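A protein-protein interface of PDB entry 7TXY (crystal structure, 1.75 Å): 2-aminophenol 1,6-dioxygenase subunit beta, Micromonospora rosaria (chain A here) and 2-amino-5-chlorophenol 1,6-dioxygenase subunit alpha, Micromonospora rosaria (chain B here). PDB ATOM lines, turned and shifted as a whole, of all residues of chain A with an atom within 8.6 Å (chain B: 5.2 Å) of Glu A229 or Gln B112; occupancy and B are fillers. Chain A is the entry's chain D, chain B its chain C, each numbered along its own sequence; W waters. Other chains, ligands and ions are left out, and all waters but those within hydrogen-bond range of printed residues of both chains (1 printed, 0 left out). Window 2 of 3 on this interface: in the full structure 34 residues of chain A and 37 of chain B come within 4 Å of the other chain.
The side-chain amide oxygen (OE1) of Gln B112 is in hydrogen-bond range of the backbone NH (N) of Glu A230, at 2.9 Å. The guanidinium group of Arg B114 is in hydrogen-bond range of the backbone carbonyl oxygen of Ile A115, 2.6 Å away. The guanidinium group (NH2) of Arg B114 sits close to a ring nitrogen (ND1) of His A118 (3.5 Å).
The backbone carbonyl oxygen of Leu B61 is in hydrogen-bond range of the guanidinium group of Arg B114, at 3.0 Å. The indole nitrogen of Trp A227 is in hydrogen-bond range of the backbone carbonyl oxygen of Arg A239, 3.3 Å away. O of Ile A309 sits at hydrogen-bond distance from N of Trp A227 (3.1 Å). The backbone NH of His B63 sits at hydrogen-bond distance from the backbone carbonyl oxygen of Gln B112 (2.9 Å). A ring nitrogen (NE2) of His A118 lies within hydrogen-bond range of the side-chain carboxylate (OE2) of Glu A230 (2.6 Å). The backbone NH of Arg B114 is in hydrogen-bond range of the backbone carbonyl oxygen of His B63, at 2.8 Å.
Among the printed residues, merely in contact across the chains: Ile A115 with Leu B61, Phe A116 with Leu B61, Trp A227 with Leu B61, His A228 with Leu B61, His A228 with Gly B62, Glu A229 with Leu B61, Glu A229 with Gly B110, Glu A229 with Gln B112 and Glu A230 with Leu B61.
Of chain B, only Leu B61 (3.8 Å), Gly B110 (3.7 Å) and Gln B112 (3.7 Å) come within 4 Å of Glu A229. Gln B112 touches two residues of chain A. No residue of chain A comes within 4 Å of Ala B113. Printed residues of chain B within 4 Å of Trp A227: Leu B61 (3.7 Å). Of the printed residues of chain B, His A118 touches Arg B114 (3.2 Å). Of the printed residues of chain B, Phe A116 touches Leu B61 (3.3 Å). Of the printed residues of chain A, Gly B110 touches Glu A229 (3.7 Å). Of the printed residues of chain B, His A228 touches Leu B61 and Gly B62. His A226 touches none of the printed residues of chain B. Arg A239 touches none of the printed residues of chain B.
Hydrophobic or aromatic side chains of chain B within 4 Å of the printed part of chain A: Leu B61. Of the 14 printed residues of chain A, 7 touch a printed residue of chain B. Hydrophobic or aromatic side chains of chain A within 4 Å of the printed part of chain B: Ile A115, Phe A116 and His A118. Along chain A the printed residues that touch a printed residue of chain B span positions 115 to 230. Among the printed residues, no Asp or Glu carboxylate lies within 4 Å of a Lys or Arg side-chain nitrogen of the other chain.
Water W1 lies within hydrogen-bond range of N of Gly B62 and O of His A228.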
ATOM      1  N   ILE A 115     -31.409   0.265  24.916  1.00  0.00           N
ATOM      2  CA  ILE A 115     -30.740  -1.030  24.886  1.00  0.00           C
ATOM      3  C   ILE A 115     -30.603  -1.551  23.457  1.00  0.00           C
ATOM      4  O   ILE A 115     -29.633  -2.251  23.145  1.00  0.00           O
ATOM      5  CB  ILE A 115     -31.493  -2.033  25.775  1.00  0.00           C
ATOM      6  CG1 ILE A 115     -31.598  -1.496  27.212  1.00  0.00           C
ATOM      7  CG2 ILE A 115     -30.793  -3.385  25.760  1.00  0.00           C
ATOM      8  CD1 ILE A 115     -32.737  -2.090  28.007  1.00  0.00           C
ATOM      9  N   PHE A 116     -31.539  -1.206  22.577  1.00  0.00           N
ATOM     10  CA  PHE A 116     -31.506  -1.605  21.173  1.00  0.00           C
ATOM     11  C   PHE A 116     -31.562  -0.375  20.274  1.00  0.00           C
ATOM     12  O   PHE A 116     -32.431  -0.271  19.396  1.00  0.00           O
ATOM     13  CB  PHE A 116     -32.661  -2.552  20.860  1.00  0.00           C
ATOM     14  CG  PHE A 116     -32.664  -3.794  21.700  1.00  0.00           C
ATOM     15  CD1 PHE A 116     -31.963  -4.923  21.292  1.00  0.00           C
ATOM     16  CD2 PHE A 116     -33.360  -3.832  22.901  1.00  0.00           C
ATOM     17  CE1 PHE A 116     -31.962  -6.068  22.066  1.00  0.00           C
ATOM     18  CE2 PHE A 116     -33.362  -4.981  23.678  1.00  0.00           C
ATOM     19  CZ  PHE A 116     -32.660  -6.096  23.260  1.00  0.00           C
ATOM     20  N   HIS A 118     -29.708   0.315  17.858  1.00  0.00           N
ATOM     21  CA  HIS A 118     -29.489  -0.130  16.488  1.00  0.00           C
ATOM     22  C   HIS A 118     -30.754  -0.690  15.855  1.00  0.00           C
ATOM     23  O   HIS A 118     -30.757  -0.958  14.650  1.00  0.00           O
ATOM     24  CB  HIS A 118     -28.382  -1.187  16.466  1.00  0.00           C
ATOM     25  CG  HIS A 118     -28.694  -2.405  17.279  1.00  0.00           C
ATOM     26  ND1 HIS A 118     -28.833  -2.369  18.650  1.00  0.00           N
ATOM     27  CD2 HIS A 118     -28.899  -3.693  16.915  1.00  0.00           C
ATOM     28  CE1 HIS A 118     -29.113  -3.582  19.097  1.00  0.00           C
ATOM     29  NE2 HIS A 118     -29.157  -4.403  18.064  1.00  0.00           N
ATOM     30  N   HIS A 226     -34.188 -13.691  28.480  1.00  0.00           N
ATOM     31  CA  HIS A 226     -33.734 -13.428  27.122  1.00  0.00           C
ATOM     32  C   HIS A 226     -32.248 -13.711  27.004  1.00  0.00           C
ATOM     33  O   HIS A 226     -31.553 -13.939  27.991  1.00  0.00           O
ATOM     34  CB  HIS A 226     -34.006 -11.974  26.724  1.00  0.00           C
ATOM     35  CG  HIS A 226     -33.447 -10.981  27.695  1.00  0.00           C
ATOM     36  ND1 HIS A 226     -32.139 -10.545  27.643  1.00  0.00           N
ATOM     37  CD2 HIS A 226     -34.008 -10.362  28.758  1.00  0.00           C
ATOM     38  CE1 HIS A 226     -31.927  -9.684  28.625  1.00  0.00           C
ATOM     39  NE2 HIS A 226     -33.044  -9.558  29.317  1.00  0.00           N
ATOM     40  N   TRP A 227     -31.762 -13.664  25.761  1.00  0.00           N
ATOM     41  CA  TRP A 227     -30.346 -13.869  25.499  1.00  0.00           C
ATOM     42  C   TRP A 227     -29.504 -12.848  26.253  1.00  0.00           C
ATOM     43  O   TRP A 227     -29.865 -11.671  26.352  1.00  0.00           O
ATOM     44  CB  TRP A 227     -30.058 -13.750  24.000  1.00  0.00           C
ATOM     45  CG  TRP A 227     -30.935 -14.583  23.107  1.00  0.00           C
ATOM     46  CD1 TRP A 227     -31.298 -14.292  21.817  1.00  0.00           C
ATOM     47  CD2 TRP A 227     -31.546 -15.845  23.419  1.00  0.00           C
ATOM     48  NE1 TRP A 227     -32.095 -15.292  21.309  1.00  0.00           N
ATOM     49  CE2 TRP A 227     -32.263 -16.258  22.271  1.00  0.00           C
ATOM     50  CE3 TRP A 227     -31.555 -16.665  24.546  1.00  0.00           C
ATOM     51  CZ2 TRP A 227     -32.987 -17.445  22.232  1.00  0.00           C
ATOM     52  CZ3 TRP A 227     -32.273 -17.847  24.501  1.00  0.00           C
ATOM     53  CH2 TRP A 227     -32.977 -18.226  23.353  1.00  0.00           C
ATOM     54  N   HIS A 228     -28.371 -13.306  26.789  1.00  0.00           N
ATOM     55  CA  HIS A 228     -27.386 -12.388  27.349  1.00  0.00           C
ATOM     56  C   HIS A 228     -26.496 -11.783  26.271  1.00  0.00           C
ATOM     57  O   HIS A 228     -25.836 -10.770  26.524  1.00  0.00           O
ATOM     58  CB  HIS A 228     -26.517 -13.106  28.386  1.00  0.00           C
ATOM     59  CG  HIS A 228     -27.261 -13.533  29.615  1.00  0.00           C
ATOM     60  ND1 HIS A 228     -28.100 -14.627  29.638  1.00  0.00           N
ATOM     61  CD2 HIS A 228     -27.282 -13.016  30.868  1.00  0.00           C
ATOM     62  CE1 HIS A 228     -28.610 -14.765  30.850  1.00  0.00           C
ATOM     63  NE2 HIS A 228     -28.128 -13.800  31.616  1.00  0.00           N
ATOM     64  N   GLU A 229     -26.473 -12.381  25.081  1.00  0.00           N
ATOM     65  CA  GLU A 229     -25.665 -11.919  23.963  1.00  0.00           C
ATOM     66  C   GLU A 229     -26.539 -11.842  22.721  1.00  0.00           C
ATOM     67  O   GLU A 229     -27.351 -12.735  22.468  1.00  0.00           O
ATOM     68  CB  GLU A 229     -24.485 -12.860  23.707  1.00  0.00           C
ATOM     69  CG  GLU A 229     -23.294 -12.626  24.614  1.00  0.00           C
ATOM     70  CD  GLU A 229     -22.036 -13.282  24.084  1.00  0.00           C
ATOM     71  OE1 GLU A 229     -22.158 -14.223  23.269  1.00  0.00           O
ATOM     72  OE2 GLU A 229     -20.930 -12.855  24.480  1.00  0.00           O
ATOM     73  N   GLU A 230     -26.366 -10.784  21.947  1.00  0.00           N
ATOM     74  CA  GLU A 230     -27.126 -10.665  20.709  1.00  0.00           C
ATOM     75  C   GLU A 230     -26.436 -11.435  19.584  1.00  0.00           C
ATOM     76  O   GLU A 230     -25.213 -11.371  19.449  1.00  0.00           O
ATOM     77  CB  GLU A 230     -27.266  -9.204  20.308  1.00  0.00           C
ATOM     78  CG  GLU A 230     -28.344  -8.957  19.272  1.00  0.00           C
ATOM     79  CD  GLU A 230     -28.355  -7.529  18.772  1.00  0.00           C
ATOM     80  OE1 GLU A 230     -27.263  -6.948  18.619  1.00  0.00           O
ATOM     81  OE2 GLU A 230     -29.453  -6.990  18.533  1.00  0.00           O
ATOM     82  N   PRO A 231     -27.188 -12.166  18.764  1.00  0.00           N
ATOM     83  CA  PRO A 231     -26.574 -12.775  17.576  1.00  0.00           C
ATOM     84  C   PRO A 231     -26.012 -11.710  16.643  1.00  0.00           C
ATOM     85  O   PRO A 231     -26.471 -10.566  16.628  1.00  0.00           O
ATOM     86  CB  PRO A 231     -27.724 -13.544  16.914  1.00  0.00           C
ATOM     87  CG  PRO A 231     -28.951 -13.248  17.686  1.00  0.00           C
ATOM     88  CD  PRO A 231     -28.584 -12.589  18.973  1.00  0.00           C
ATOM     89  N   GLU A 232     -25.012 -12.106  15.848  1.00  0.00           N
ATOM     90  CA  GLU A 232     -24.337 -11.146  14.975  1.00  0.00           C
ATOM     91  C   GLU A 232     -25.324 -10.449  14.048  1.00  0.00           C
ATOM     92  O   GLU A 232     -25.219  -9.242  13.809  1.00  0.00           O
ATOM     93  CB  GLU A 232     -23.250 -11.845  14.163  1.00  0.00           C
ATOM     94  CG  GLU A 232     -22.822 -11.078  12.917  1.00  0.00           C
ATOM     95  CD  GLU A 232     -21.436 -11.468  12.436  1.00  0.00           C
ATOM     96  OE1 GLU A 232     -21.152 -12.682  12.355  1.00  0.00           O
ATOM     97  OE2 GLU A 232     -20.632 -10.559  12.138  1.00  0.00           O
ATOM     98  N   PRO A 234     -29.112  -9.509  14.119  1.00  0.00           N
ATOM     99  CA  PRO A 234     -30.250  -9.557  15.053  1.00  0.00           C
ATOM    100  C   PRO A 234     -31.418 -10.390  14.560  1.00  0.00           C
ATOM    101  O   PRO A 234     -32.028 -11.116  15.355  1.00  0.00           O
ATOM    102  CB  PRO A 234     -30.624  -8.072  15.209  1.00  0.00           C
ATOM    103  CG  PRO A 234     -29.334  -7.347  14.999  1.00  0.00           C
ATOM    104  CD  PRO A 234     -28.626  -8.129  13.913  1.00  0.00           C
ATOM    105  N   ARG A 239     -31.515 -18.339  15.357  1.00  0.00           N
ATOM    106  CA  ARG A 239     -31.191 -18.084  16.754  1.00  0.00           C
ATOM    107  C   ARG A 239     -32.391 -17.623  17.565  1.00  0.00           C
ATOM    108  O   ARG A 239     -32.235 -17.301  18.747  1.00  0.00           O
ATOM    109  CB  ARG A 239     -30.071 -17.039  16.833  1.00  0.00           C
ATOM    110  CG  ARG A 239     -28.733 -17.540  16.303  1.00  0.00           C
ATOM    111  CD  ARG A 239     -27.944 -18.259  17.388  1.00  0.00           C
ATOM    112  NE  ARG A 239     -27.294 -17.311  18.288  1.00  0.00           N
ATOM    113  CZ  ARG A 239     -26.168 -16.667  18.012  1.00  0.00           C
ATOM    114  NH1 ARG A 239     -25.519 -16.866  16.875  1.00  0.00           N
ATOM    115  NH2 ARG A 239     -25.681 -15.801  18.897  1.00  0.00           N
ATOM    116  N   TYR A 243     -36.462 -19.303  25.281  1.00  0.00           N
ATOM    117  CA  TYR A 243     -35.335 -19.329  26.208  1.00  0.00           C
ATOM    118  C   TYR A 243     -35.096 -20.745  26.722  1.00  0.00           C
ATOM    119  O   TYR A 243     -33.962 -21.236  26.728  1.00  0.00           O
ATOM    120  CB  TYR A 243     -35.602 -18.355  27.364  1.00  0.00           C
ATOM    121  CG  TYR A 243     -34.456 -18.204  28.340  1.00  0.00           C
ATOM    122  CD1 TYR A 243     -33.396 -17.352  28.073  1.00  0.00           C
ATOM    123  CD2 TYR A 243     -34.445 -18.909  29.535  1.00  0.00           C
ATOM    124  CE1 TYR A 243     -32.345 -17.214  28.969  1.00  0.00           C
ATOM    125  CE2 TYR A 243     -33.404 -18.779  30.430  1.00  0.00           C
ATOM    126  CZ  TYR A 243     -32.360 -17.931  30.147  1.00  0.00           C
ATOM    127  OH  TYR A 243     -31.326 -17.804  31.044  1.00  0.00           O
ATOM    128  N   ILE A 309     -35.793 -12.658  21.061  1.00  0.00           N
ATOM    129  CA  ILE A 309     -34.588 -12.967  21.831  1.00  0.00           C
ATOM    130  C   ILE A 309     -34.919 -13.887  23.003  1.00  0.00           C
ATOM    131  O   ILE A 309     -34.389 -13.722  24.106  1.00  0.00           O
ATOM    132  CB  ILE A 309     -33.866 -11.690  22.314  1.00  0.00           C
ATOM    133  CG1 ILE A 309     -34.789 -10.784  23.134  1.00  0.00           C
ATOM    134  CG2 ILE A 309     -33.284 -10.937  21.116  1.00  0.00           C
ATOM    135  CD1 ILE A 309     -34.061  -9.682  23.872  1.00  0.00           C
ATOM    136  N   LEU B  61     -28.429  -6.195  27.998  1.00  0.00           N
ATOM    137  CA  LEU B  61     -27.815  -6.901  26.874  1.00  0.00           C
ATOM    138  C   LEU B  61     -26.395  -6.388  26.706  1.00  0.00           C
ATOM    139  O   LEU B  61     -26.189  -5.257  26.251  1.00  0.00           O
ATOM    140  CB  LEU B  61     -28.625  -6.705  25.595  1.00  0.00           C
ATOM    141  CG  LEU B  61     -28.119  -7.412  24.339  1.00  0.00           C
ATOM    142  CD1 LEU B  61     -28.170  -8.925  24.517  1.00  0.00           C
ATOM    143  CD2 LEU B  61     -28.950  -6.982  23.140  1.00  0.00           C
ATOM    144  N   GLY B  62     -25.423  -7.210  27.078  1.00  0.00           N
ATOM    145  CA  GLY B  62     -24.052  -6.797  26.958  1.00  0.00           C
ATOM    146  C   GLY B  62     -23.760  -5.554  27.790  1.00  0.00           C
ATOM    147  O   GLY B  62     -24.455  -5.222  28.756  1.00  0.00           O
ATOM    148  N   HIS B  63     -22.703  -4.852  27.385  1.00  0.00           N
ATOM    149  CA  HIS B  63     -22.222  -3.669  28.087  1.00  0.00           C
ATOM    150  C   HIS B  63     -22.041  -2.562  27.063  1.00  0.00           C
ATOM    151  O   HIS B  63     -21.195  -2.662  26.170  1.00  0.00           O
ATOM    152  CB  HIS B  63     -20.926  -3.973  28.834  1.00  0.00           C
ATOM    153  CG  HIS B  63     -21.035  -5.139  29.770  1.00  0.00           C
ATOM    154  ND1 HIS B  63     -21.544  -5.024  31.045  1.00  0.00           N
ATOM    155  CD2 HIS B  63     -20.716  -6.444  29.608  1.00  0.00           C
ATOM    156  CE1 HIS B  63     -21.522  -6.208  31.632  1.00  0.00           C
ATOM    157  NE2 HIS B  63     -21.025  -7.086  30.783  1.00  0.00           N
ATOM    158  N   VAL B 106     -12.870  -5.255  27.284  1.00  0.00           N
ATOM    159  CA  VAL B 106     -14.066  -5.985  27.692  1.00  0.00           C
ATOM    160  C   VAL B 106     -14.404  -7.058  26.660  1.00  0.00           C
ATOM    161  O   VAL B 106     -14.745  -8.193  27.013  1.00  0.00           O
ATOM    162  CB  VAL B 106     -15.237  -5.008  27.906  1.00  0.00           C
ATOM    163  CG1 VAL B 106     -16.543  -5.751  28.061  1.00  0.00           C
ATOM    164  CG2 VAL B 106     -14.968  -4.132  29.121  1.00  0.00           C
ATOM    165  N   GLN B 107     -14.313  -6.716  25.372  1.00  0.00           N
ATOM    166  CA  GLN B 107     -14.563  -7.701  24.322  1.00  0.00           C
ATOM    167  C   GLN B 107     -13.534  -8.824  24.375  1.00  0.00           C
ATOM    168  O   GLN B 107     -13.881 -10.003  24.226  1.00  0.00           O
ATOM    169  CB  GLN B 107     -14.551  -7.019  22.954  1.00  0.00           C
ATOM    170  CG  GLN B 107     -15.172  -7.836  21.822  1.00  0.00           C
ATOM    171  CD  GLN B 107     -16.634  -8.174  22.065  1.00  0.00           C
ATOM    172  OE1 GLN B 107     -17.512  -7.311  21.973  1.00  0.00           O
ATOM    173  NE2 GLN B 107     -16.904  -9.438  22.376  1.00  0.00           N
ATOM    174  N   GLY B 110     -14.274 -11.820  26.601  1.00  0.00           N
ATOM    175  CA  GLY B 110     -15.412 -12.666  26.321  1.00  0.00           C
ATOM    176  C   GLY B 110     -16.767 -12.038  26.548  1.00  0.00           C
ATOM    177  O   GLY B 110     -17.778 -12.739  26.451  1.00  0.00           O
ATOM    178  N   MET B 111     -16.823 -10.748  26.853  1.00  0.00           N
ATOM    179  CA  MET B 111     -18.077 -10.038  27.057  1.00  0.00           C
ATOM    180  C   MET B 111     -18.420  -9.229  25.814  1.00  0.00           C
ATOM    181  O   MET B 111     -17.549  -8.855  25.029  1.00  0.00           O
ATOM    182  CB  MET B 111     -17.984  -9.119  28.275  1.00  0.00           C
ATOM    183  CG  MET B 111     -17.801  -9.856  29.589  1.00  0.00           C
ATOM    184  SD  MET B 111     -17.470  -8.757  30.985  1.00  0.00           S
ATOM    185  CE  MET B 111     -15.698  -8.572  30.860  1.00  0.00           C
ATOM    186  N   GLN B 112     -19.713  -8.965  25.636  1.00  0.00           N
ATOM    187  CA  GLN B 112     -20.201  -8.227  24.473  1.00  0.00           C
ATOM    188  C   GLN B 112     -20.096  -6.734  24.767  1.00  0.00           C
ATOM    189  O   GLN B 112     -20.937  -6.171  25.468  1.00  0.00           O
ATOM    190  CB  GLN B 112     -21.634  -8.622  24.142  1.00  0.00           C
ATOM    191  CG  GLN B 112     -22.084  -8.205  22.749  1.00  0.00           C
ATOM    192  CD  GLN B 112     -23.293  -8.986  22.263  1.00  0.00           C
ATOM    193  OE1 GLN B 112     -24.431  -8.685  22.625  1.00  0.00           O
ATOM    194  NE2 GLN B 112     -23.048  -9.999  21.438  1.00  0.00           N
ATOM    195  N   ALA B 113     -19.060  -6.094  24.227  1.00  0.00           N
ATOM    196  CA  ALA B 113     -18.902  -4.648  24.322  1.00  0.00           C
ATOM    197  C   ALA B 113     -19.616  -4.007  23.142  1.00  0.00           C
ATOM    198  O   ALA B 113     -19.341  -4.342  21.983  1.00  0.00           O
ATOM    199  CB  ALA B 113     -17.427  -4.261  24.338  1.00  0.00           C
ATOM    200  N   ARG B 114     -20.530  -3.087  23.432  1.00  0.00           N
ATOM    201  CA  ARG B 114     -21.401  -2.498  22.418  1.00  0.00           C
ATOM    202  C   ARG B 114     -21.141  -1.001  22.366  1.00  0.00           C
ATOM    203  O   ARG B 114     -21.441  -0.277  23.326  1.00  0.00           O
ATOM    204  CB  ARG B 114     -22.864  -2.806  22.720  1.00  0.00           C
ATOM    205  CG  ARG B 114     -23.154  -4.295  22.813  1.00  0.00           C
ATOM    206  CD  ARG B 114     -24.571  -4.565  23.291  1.00  0.00           C
ATOM    207  NE  ARG B 114     -25.558  -4.017  22.369  1.00  0.00           N
ATOM    208  CZ  ARG B 114     -26.726  -3.504  22.728  1.00  0.00           C
ATOM    209  NH1 ARG B 114     -27.112  -3.478  23.996  1.00  0.00           N
ATOM    210  NH2 ARG B 114     -27.526  -3.007  21.791  1.00  0.00           N
HETATM  211  O   HOH W   1     -26.608  -9.188  29.506  1.00  0.00           O
